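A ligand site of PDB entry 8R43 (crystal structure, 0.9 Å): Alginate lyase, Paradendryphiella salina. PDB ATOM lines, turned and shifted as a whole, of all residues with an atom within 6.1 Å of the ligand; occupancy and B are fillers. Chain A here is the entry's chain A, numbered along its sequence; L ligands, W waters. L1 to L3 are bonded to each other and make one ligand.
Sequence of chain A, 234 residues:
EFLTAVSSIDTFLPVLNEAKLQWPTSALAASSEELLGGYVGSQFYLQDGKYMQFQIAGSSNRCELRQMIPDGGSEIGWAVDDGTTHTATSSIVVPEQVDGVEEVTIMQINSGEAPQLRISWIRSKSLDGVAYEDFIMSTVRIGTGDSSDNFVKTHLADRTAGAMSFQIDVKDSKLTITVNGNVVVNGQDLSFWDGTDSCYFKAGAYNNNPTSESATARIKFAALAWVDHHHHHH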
ATOM      1  N   SER A  60      19.564 -16.308 -23.953  1.00  0.00           N
ATOM      2  CA  SER A  60      20.410 -15.185 -23.578  1.00  0.00           C
ATOM      3  C   SER A  60      19.976 -13.864 -24.195  1.00  0.00           C
ATOM      4  O   SER A  60      20.730 -12.883 -24.132  1.00  0.00           O
ATOM      5  CB  SER A  60      21.894 -15.461 -23.829  1.00  0.00           C
ATOM      6  OG  SER A  60      22.310 -16.521 -22.988  1.00  0.00           O
ATOM      7  N   GLU A 103      15.011 -19.748 -16.298  1.00  0.00           N
ATOM      8  CA  GLU A 103      15.648 -18.785 -15.422  1.00  0.00           C
ATOM      9  C   GLU A 103      15.518 -17.426 -16.085  1.00  0.00           C
ATOM     10  O   GLU A 103      15.808 -17.296 -17.269  1.00  0.00           O
ATOM     11  CB  GLU A 103      17.116 -19.115 -15.160  1.00  0.00           C
ATOM     12  CG  GLU A 103      17.772 -18.031 -14.267  1.00  0.00           C
ATOM     13  CD  GLU A 103      19.200 -18.308 -13.827  1.00  0.00           C
ATOM     14  OE1 GLU A 103      19.862 -19.188 -14.411  1.00  0.00           O
ATOM     15  OE2 GLU A 103      19.655 -17.605 -12.888  1.00  0.00           O
ATOM     16  N   THR A 105      16.687 -13.479 -15.297  1.00  0.00           N
ATOM     17  CA  THR A 105      17.359 -12.474 -14.490  1.00  0.00           C
ATOM     18  C   THR A 105      16.568 -11.187 -14.545  1.00  0.00           C
ATOM     19  O   THR A 105      16.264 -10.683 -15.641  1.00  0.00           O
ATOM     20  CB  THR A 105      18.789 -12.286 -14.981  1.00  0.00           C
ATOM     21  OG1 THR A 105      19.531 -13.491 -14.781  1.00  0.00           O
ATOM     22  CG2 THR A 105      19.484 -11.162 -14.264  1.00  0.00           C
ATOM     23  N   GLN A 108      20.317  -6.858 -11.795  1.00  0.00           N
ATOM     24  CA  GLN A 108      21.738  -7.190 -11.776  1.00  0.00           C
ATOM     25  C   GLN A 108      22.567  -6.042 -11.225  1.00  0.00           C
ATOM     26  O   GLN A 108      22.178  -4.884 -11.293  1.00  0.00           O
ATOM     27  CB  GLN A 108      22.319  -7.456 -13.176  1.00  0.00           C
ATOM     28  CG  GLN A 108      21.544  -8.475 -13.998  1.00  0.00           C
ATOM     29  CD  GLN A 108      22.370  -9.003 -15.153  1.00  0.00           C
ATOM     30  OE1 GLN A 108      23.438  -9.557 -14.956  1.00  0.00           O
ATOM     31  NE2 GLN A 108      21.876  -8.846 -16.372  1.00  0.00           N
ATOM     32  N   ALA A 114      32.541  -9.133 -15.087  1.00  0.00           N
ATOM     33  CA  ALA A 114      31.655 -10.278 -14.883  1.00  0.00           C
ATOM     34  C   ALA A 114      30.486  -9.766 -14.056  1.00  0.00           C
ATOM     35  O   ALA A 114      30.593  -8.677 -13.469  1.00  0.00           O
ATOM     36  CB  ALA A 114      32.343 -11.426 -14.135  1.00  0.00           C
ATOM     37  N   PRO A 115      29.365 -10.493 -13.977  1.00  0.00           N
ATOM     38  CA  PRO A 115      28.256  -9.992 -13.164  1.00  0.00           C
ATOM     39  C   PRO A 115      28.532 -10.214 -11.689  1.00  0.00           C
ATOM     40  O   PRO A 115      28.664 -11.352 -11.233  1.00  0.00           O
ATOM     41  CB  PRO A 115      27.060 -10.814 -13.649  1.00  0.00           C
ATOM     42  CG  PRO A 115      27.640 -12.077 -14.146  1.00  0.00           C
ATOM     43  CD  PRO A 115      28.991 -11.704 -14.733  1.00  0.00           C
ATOM     44  N   ARG A 118      23.344 -11.325  -9.807  1.00  0.00           N
ATOM     45  CA  ARG A 118      22.062 -11.458 -10.493  1.00  0.00           C
ATOM     46  C   ARG A 118      21.006 -11.885  -9.491  1.00  0.00           C
ATOM     47  O   ARG A 118      21.236 -12.772  -8.656  1.00  0.00           O
ATOM     48  CB  ARG A 118      22.121 -12.505 -11.613  1.00  0.00           C
ATOM     49  CG  ARG A 118      23.152 -12.181 -12.667  1.00  0.00           C
ATOM     50  CD  ARG A 118      23.120 -13.148 -13.845  1.00  0.00           C
ATOM     51  NE  ARG A 118      23.398 -14.514 -13.420  1.00  0.00           N
ATOM     52  CZ  ARG A 118      22.492 -15.445 -13.170  1.00  0.00           C
ATOM     53  NH1 ARG A 118      21.211 -15.267 -13.463  1.00  0.00           N
ATOM     54  NH2 ARG A 118      22.874 -16.605 -12.630  1.00  0.00           N
ATOM     55  N   LYS A 125      15.687 -25.806  -8.583  1.00  0.00           N
ATOM     56  CA  LYS A 125      17.104 -25.913  -8.277  1.00  0.00           C
ATOM     57  C   LYS A 125      17.292 -26.381  -6.847  1.00  0.00           C
ATOM     58  O   LYS A 125      16.545 -25.986  -5.950  1.00  0.00           O
ATOM     59  CB  LYS A 125      17.828 -24.590  -8.458  1.00  0.00           C
ATOM     60  CG  LYS A 125      19.325 -24.766  -8.613  1.00  0.00           C
ATOM     61  CD  LYS A 125      19.977 -23.452  -8.940  1.00  0.00           C
ATOM     62  CE  LYS A 125      21.476 -23.585  -8.980  1.00  0.00           C
ATOM     63  NZ  LYS A 125      21.844 -24.604  -9.994  1.00  0.00           N
ATOM     64  N   SER A 126      18.314 -27.202  -6.635  1.00  0.00           N
ATOM     65  CA  SER A 126      18.751 -27.581  -5.302  1.00  0.00           C
ATOM     66  C   SER A 126      19.894 -26.661  -4.887  1.00  0.00           C
ATOM     67  O   SER A 126      20.828 -26.442  -5.655  1.00  0.00           O
ATOM     68  CB  SER A 126      19.227 -29.033  -5.313  1.00  0.00           C
ATOM     69  OG  SER A 126      19.582 -29.434  -4.003  1.00  0.00           O
ATOM     70  N   LEU A 127      19.792 -26.132  -3.668  1.00  0.00           N
ATOM     71  CA  LEU A 127      20.810 -25.261  -3.106  1.00  0.00           C
ATOM     72  C   LEU A 127      21.172 -25.785  -1.722  1.00  0.00           C
ATOM     73  O   LEU A 127      20.310 -25.882  -0.843  1.00  0.00           O
ATOM     74  CB  LEU A 127      20.296 -23.826  -2.966  1.00  0.00           C
ATOM     75  CG  LEU A 127      20.002 -23.098  -4.280  1.00  0.00           C
ATOM     76  CD1 LEU A 127      19.374 -21.737  -4.012  1.00  0.00           C
ATOM     77  CD2 LEU A 127      21.258 -22.918  -5.107  1.00  0.00           C
ATOM     78  N   MET A 137      16.171 -16.145  -6.618  1.00  0.00           N
ATOM     79  CA  MET A 137      17.515 -16.499  -6.192  1.00  0.00           C
ATOM     80  C   MET A 137      18.449 -15.311  -6.383  1.00  0.00           C
ATOM     81  O   MET A 137      18.267 -14.528  -7.317  1.00  0.00           O
ATOM     82  CB  MET A 137      18.015 -17.667  -7.069  1.00  0.00           C
ATOM     83  CG  MET A 137      19.285 -18.333  -6.581  1.00  0.00           C
ATOM     84  SD  MET A 137      19.658 -19.867  -7.452  1.00  0.00           S
ATOM     85  CE  MET A 137      20.201 -19.254  -9.044  1.00  0.00           C
ATOM     86  N   THR A 139      22.590 -14.738  -7.157  1.00  0.00           N
ATOM     87  CA  THR A 139      23.856 -15.334  -7.562  1.00  0.00           C
ATOM     88  C   THR A 139      24.904 -14.239  -7.484  1.00  0.00           C
ATOM     89  O   THR A 139      24.839 -13.257  -8.232  1.00  0.00           O
ATOM     90  CB  THR A 139      23.786 -15.886  -8.986  1.00  0.00           C
ATOM     91  OG1 THR A 139      22.777 -16.892  -9.070  1.00  0.00           O
ATOM     92  CG2 THR A 139      25.102 -16.485  -9.401  1.00  0.00           C
ATOM     93  N   ARG A 141      29.014 -13.384  -7.647  1.00  0.00           N
ATOM     94  CA  ARG A 141      30.335 -13.874  -8.005  1.00  0.00           C
ATOM     95  C   ARG A 141      31.371 -13.468  -6.976  1.00  0.00           C
ATOM     96  O   ARG A 141      31.465 -12.292  -6.605  1.00  0.00           O
ATOM     97  CB  ARG A 141      30.786 -13.398  -9.384  1.00  0.00           C
ATOM     98  CG  ARG A 141      30.325 -14.298 -10.518  1.00  0.00           C
ATOM     99  CD  ARG A 141      30.905 -13.814 -11.845  1.00  0.00           C
ATOM    100  NE  ARG A 141      30.691 -14.749 -12.929  1.00  0.00           N
ATOM    101  CZ  ARG A 141      31.480 -15.772 -13.205  1.00  0.00           C
ATOM    102  NH1 ARG A 141      32.574 -16.009 -12.515  1.00  0.00           N
ATOM    103  NH2 ARG A 141      31.176 -16.565 -14.227  1.00  0.00           N
ATOM    104  N   ASP A 146      34.374 -20.520 -13.683  1.00  0.00           N
ATOM    105  CA  ASP A 146      33.077 -21.056 -14.067  1.00  0.00           C
ATOM    106  C   ASP A 146      32.508 -22.078 -13.096  1.00  0.00           C
ATOM    107  O   ASP A 146      31.292 -22.295 -13.091  1.00  0.00           O
ATOM    108  CB  ASP A 146      33.181 -21.729 -15.449  1.00  0.00           C
ATOM    109  CG  ASP A 146      34.080 -20.973 -16.412  1.00  0.00           C
ATOM    110  OD1 ASP A 146      33.765 -19.800 -16.709  1.00  0.00           O
ATOM    111  OD2 ASP A 146      35.111 -21.536 -16.859  1.00  0.00           O
ATOM    112  N   SER A 147      33.346 -22.712 -12.279  1.00  0.00           N
ATOM    113  CA  SER A 147      32.860 -23.722 -11.362  1.00  0.00           C
ATOM    114  C   SER A 147      32.045 -23.071 -10.241  1.00  0.00           C
ATOM    115  O   SER A 147      32.130 -21.877  -9.980  1.00  0.00           O
ATOM    116  CB  SER A 147      34.029 -24.474 -10.741  1.00  0.00           C
ATOM    117  OG  SER A 147      34.787 -23.595  -9.940  1.00  0.00           O
ATOM    118  N   SER A 148      31.291 -23.922  -9.539  1.00  0.00           N
ATOM    119  CA  SER A 148      30.359 -23.432  -8.510  1.00  0.00           C
ATOM    120  C   SER A 148      31.067 -22.670  -7.404  1.00  0.00           C
ATOM    121  O   SER A 148      30.451 -21.825  -6.754  1.00  0.00           O
ATOM    122  CB  SER A 148      29.589 -24.609  -7.917  1.00  0.00           C
ATOM    123  OG  SER A 148      30.432 -25.428  -7.147  1.00  0.00           O
ATOM    124  N   PHE A 151      30.769 -18.799  -7.063  1.00  0.00           N
ATOM    125  CA  PHE A 151      29.471 -18.177  -6.845  1.00  0.00           C
ATOM    126  C   PHE A 151      28.951 -18.486  -5.453  1.00  0.00           C
ATOM    127  O   PHE A 151      29.232 -19.539  -4.878  1.00  0.00           O
ATOM    128  CB  PHE A 151      28.427 -18.709  -7.830  1.00  0.00           C
ATOM    129  CG  PHE A 151      28.849 -18.637  -9.263  1.00  0.00           C
ATOM    130  CD1 PHE A 151      29.550 -19.678  -9.852  1.00  0.00           C
ATOM    131  CD2 PHE A 151      28.559 -17.530 -10.043  1.00  0.00           C
ATOM    132  CE1 PHE A 151      29.939 -19.616 -11.176  1.00  0.00           C
ATOM    133  CE2 PHE A 151      28.958 -17.467 -11.369  1.00  0.00           C
ATOM    134  CZ  PHE A 151      29.653 -18.497 -11.923  1.00  0.00           C
ATOM    135  N   LYS A 153      25.080 -18.717  -4.162  1.00  0.00           N
ATOM    136  CA  LYS A 153      23.690 -18.721  -4.586  1.00  0.00           C
ATOM    137  C   LYS A 153      22.799 -18.892  -3.363  1.00  0.00           C
ATOM    138  O   LYS A 153      23.090 -19.714  -2.480  1.00  0.00           O
ATOM    139  CB  LYS A 153      23.450 -19.814  -5.631  1.00  0.00           C
ATOM    140  CG  LYS A 153      24.331 -19.595  -6.881  1.00  0.00           C
ATOM    141  CD  LYS A 153      24.019 -20.546  -8.014  1.00  0.00           C
ATOM    142  CE  LYS A 153      24.817 -20.223  -9.254  1.00  0.00           C
ATOM    143  NZ  LYS A 153      24.579 -21.251 -10.305  1.00  0.00           N
ATOM    144  N   TYR A 206      16.107 -10.945 -18.578  1.00  0.00           N
ATOM    145  CA  TYR A 206      17.230 -11.521 -19.297  1.00  0.00           C
ATOM    146  C   TYR A 206      17.078 -13.035 -19.196  1.00  0.00           C
ATOM    147  O   TYR A 206      17.063 -13.597 -18.098  1.00  0.00           O
ATOM    148  CB  TYR A 206      18.528 -10.986 -18.714  1.00  0.00           C
ATOM    149  CG  TYR A 206      19.810 -11.641 -19.126  1.00  0.00           C
ATOM    150  CD1 TYR A 206      20.043 -12.097 -20.425  1.00  0.00           C
ATOM    151  CD2 TYR A 206      20.837 -11.714 -18.215  1.00  0.00           C
ATOM    152  CE1 TYR A 206      21.263 -12.651 -20.769  1.00  0.00           C
ATOM    153  CE2 TYR A 206      22.057 -12.251 -18.544  1.00  0.00           C
ATOM    154  CZ  TYR A 206      22.264 -12.715 -19.819  1.00  0.00           C
ATOM    155  OH  TYR A 206      23.483 -13.252 -20.149  1.00  0.00           O
ATOM    156  N   ASN A 208      17.733 -16.827 -19.406  1.00  0.00           N
ATOM    157  CA  ASN A 208      18.926 -17.666 -19.230  1.00  0.00           C
ATOM    158  C   ASN A 208      18.569 -19.139 -19.426  1.00  0.00           C
ATOM    159  O   ASN A 208      17.704 -19.667 -18.727  1.00  0.00           O
ATOM    160  CB  ASN A 208      19.536 -17.468 -17.828  1.00  0.00           C
ATOM    161  CG  ASN A 208      19.659 -16.005 -17.433  1.00  0.00           C
ATOM    162  OD1 ASN A 208      19.065 -15.562 -16.437  1.00  0.00           O
ATOM    163  ND2 ASN A 208      20.400 -15.237 -18.217  1.00  0.00           N
ATOM    164  N   ASN A 209      19.265 -19.804 -20.340  1.00  0.00           N
ATOM    165  CA  ASN A 209      19.153 -21.249 -20.522  1.00  0.00           C
ATOM    166  C   ASN A 209      17.716 -21.761 -20.729  1.00  0.00           C
ATOM    167  O   ASN A 209      17.342 -22.794 -20.162  1.00  0.00           O
ATOM    168  CB  ASN A 209      19.803 -21.983 -19.350  1.00  0.00           C
ATOM    169  CG  ASN A 209      21.251 -21.606 -19.179  1.00  0.00           C
ATOM    170  OD1 ASN A 209      22.006 -21.578 -20.140  1.00  0.00           O
ATOM    171  ND2 ASN A 209      21.637 -21.297 -17.949  1.00  0.00           N
HETATM  172  C1  LIG L   1      25.355 -14.135 -17.596  1.00  0.00           C
HETATM  173  O1  LIG L   1      24.772 -13.336 -16.764  1.00  0.00           O
HETATM  174  C2  LIG L   1      24.413 -15.357 -17.747  1.00  0.00           C
HETATM  175  O2  LIG L   1      24.847 -16.166 -18.826  1.00  0.00           O
HETATM  176  C3  LIG L   1      24.371 -16.194 -16.524  1.00  0.00           C
HETATM  177  O3  LIG L   1      23.530 -17.370 -16.776  1.00  0.00           O
HETATM  178  C4  LIG L   1      25.744 -16.533 -16.026  1.00  0.00           C
HETATM  179  O4  LIG L   1      25.565 -17.179 -14.740  1.00  0.00           O
HETATM  180  C5  LIG L   1      26.559 -15.285 -15.814  1.00  0.00           C
HETATM  181  O5  LIG L   1      26.735 -14.574 -17.072  1.00  0.00           O
HETATM  182  C6  LIG L   1      27.963 -15.487 -15.276  1.00  0.00           C
HETATM  183  O6  LIG L   1      28.147 -15.352 -14.041  1.00  0.00           O
HETATM  184  O7  LIG L   1      28.903 -15.740 -16.059  1.00  0.00           O
HETATM  185  C1  LG2 L   2      26.232 -18.427 -14.599  1.00  0.00           C
HETATM  186  C2  LG2 L   2      26.174 -18.909 -13.190  1.00  0.00           C
HETATM  187  O1  LG2 L   2      24.796 -18.924 -12.749  1.00  0.00           O
HETATM  188  C3  LG2 L   2      26.743 -20.280 -13.125  1.00  0.00           C
HETATM  189  O2  LG2 L   2      26.737 -20.746 -11.763  1.00  0.00           O
HETATM  190  C4  LG2 L   2      25.979 -21.252 -13.969  1.00  0.00           C
HETATM  191  O3  LG2 L   2      26.601 -22.542 -13.956  1.00  0.00           O
HETATM  192  C5  LG2 L   2      25.992 -20.758 -15.398  1.00  0.00           C
HETATM  193  O4  LG2 L   2      25.569 -19.376 -15.498  1.00  0.00           O
HETATM  194  C6  LG2 L   2      25.035 -21.592 -16.193  1.00  0.00           C
HETATM  195  O5  LG2 L   2      25.488 -22.524 -16.918  1.00  0.00           O
HETATM  196  O6  LG2 L   2      23.804 -21.353 -16.114  1.00  0.00           O
HETATM  197  C1  LG3 L   3      25.705 -23.600 -13.614  1.00  0.00           C
HETATM  198  C2  LG3 L   3      26.291 -24.904 -14.111  1.00  0.00           C
HETATM  199  O1  LG3 L   3      27.622 -25.058 -13.538  1.00  0.00           O
HETATM  200  C3  LG3 L   3      25.420 -26.040 -13.741  1.00  0.00           C
HETATM  201  O2  LG3 L   3      26.024 -27.271 -14.192  1.00  0.00           O
HETATM  202  C4  LG3 L   3      25.211 -26.120 -12.255  1.00  0.00           C
HETATM  203  O3  LG3 L   3      24.251 -27.139 -11.965  1.00  0.00           O
HETATM  204  C5  LG3 L   3      24.704 -24.795 -11.694  1.00  0.00           C
HETATM  205  O4  LG3 L   3      25.446 -23.617 -12.146  1.00  0.00           O
HETATM  206  C6  LG3 L   3      24.813 -24.890 -10.209  1.00  0.00           C
HETATM  207  O5  LG3 L   3      24.578 -25.990  -9.655  1.00  0.00           O
HETATM  208  O6  LG3 L   3      25.062 -23.883  -9.502  1.00  0.00           O
HETATM  209  O   HOH W   1      22.251 -16.518 -20.201  1.00  0.00           O
HETATM  210  O   HOH W   2      24.489 -23.034 -19.499  1.00  0.00           O
HETATM  211  O   HOH W   3      21.184 -27.083 -12.637  1.00  0.00           O
HETATM  212  O   HOH W   4      21.793 -18.472 -11.565  1.00  0.00           O
HETATM  213  O   HOH W   5      29.291 -26.812 -14.580  1.00  0.00           O
HETATM  214  O   HOH W   6      31.402 -14.322 -16.819  1.00  0.00           O
HETATM  215  O   HOH W   7      22.696 -19.102 -14.738  1.00  0.00           O
HETATM  216  O   HOH W   8      25.961 -15.004 -12.406  1.00  0.00           O
HETATM  217  O   HOH W   9      28.560 -16.332 -18.751  1.00  0.00           O
HETATM  218  O   HOH W  10      29.367 -22.238 -14.814  1.00  0.00           O
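CG of Pro 115 touches O6 of LIG L1, at 3.3 Å. CE1 of Phe 151 touches O2 of LG2 L2, 3.4 Å away. Hydrophobic or aromatic side chains that line the ligand: Pro 115, Phe 151 and Tyr 206. Of the 21 residues printed, 8 come within 4 Å of the ligand. The nearest printed residue that does not touch the ligand is Asn 208 (4.04 Å).
O of Tyr 206 lies close to OD1 of Asn 208 (3.3 Å). The backbone carbonyl oxygen (O) of Tyr 206 is in hydrogen-bond range of the backbone NH (N) of Thr 105. NH1 of Arg 118 sits at hydrogen-bond distance from OG1 of Thr 105 (2.8 Å). The guanidinium group (NH1) of Arg 118 lies within salt-bridge range of the side-chain carboxylate (OE2) of Glu 103 (2.9 Å). O of Arg 118 is in hydrogen-bond range of N of Thr 139, at 2.8 Å.
Water W8 bridges O6 of LIG L1 (2.8 Å) and NE of Arg 118 (2.8 Å). Water W7 lies within hydrogen-bond range of O3 of LIG L1 (2.8 Å), OE1 of Glu 103 (2.9 Å) and NH2 of Arg 118 (3.3 Å). Water W2 bridges O5 of LG2 L2 and OD1 of Asn 209. Water W1 lies within hydrogen-bond range of the side-chain hydroxyl (OG) of Ser 60 (2.8 Å), an oxygen (O2) of LIG L1 (3.0 Å), the side-chain amide nitrogen (ND2) of Asn 208 (3.0 Å) and the side-chain hydroxyl (OH) of Tyr 206 (3.5 Å). Water W6 lies within hydrogen-bond range of an oxygen (O7) of LIG L1 (3.0 Å) and the guanidinium group of Arg 141 (3.4 Å). Water W4 lies within hydrogen-bond range of the guanidinium group of Arg 118 (2.4 Å), the side-chain carboxylate of Glu 103 (2.7 Å), the side-chain hydroxyl of Thr 139 (3.1 Å) and an oxygen (O1) of LG2 L2 (3.3 Å).
The side-chain amino group of Lys 125 lies within salt-bridge range of an oxygen (O5) of LG3 L3 (3.1 Å). The guanidinium group (NE) of Arg 141 is in salt-bridge range of an oxygen (O6) of LIG L1 (2.8 Å). The side-chain amino group of Lys 153 is in salt-bridge range of an oxygen (O6) of LG3 L3 (2.8 Å). O6 of LG2 L2 is in hydrogen-bond range of ND2 of Asn 209 (2.8 Å). The guanidinium group (NH2) of Arg 118 lies within hydrogen-bond range of an oxygen (O1) of LG2 L2 (3.0 Å). The side-chain hydroxyl of Tyr 206 sits close to an oxygen (O2) of LIG L1 (3.5 Å).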
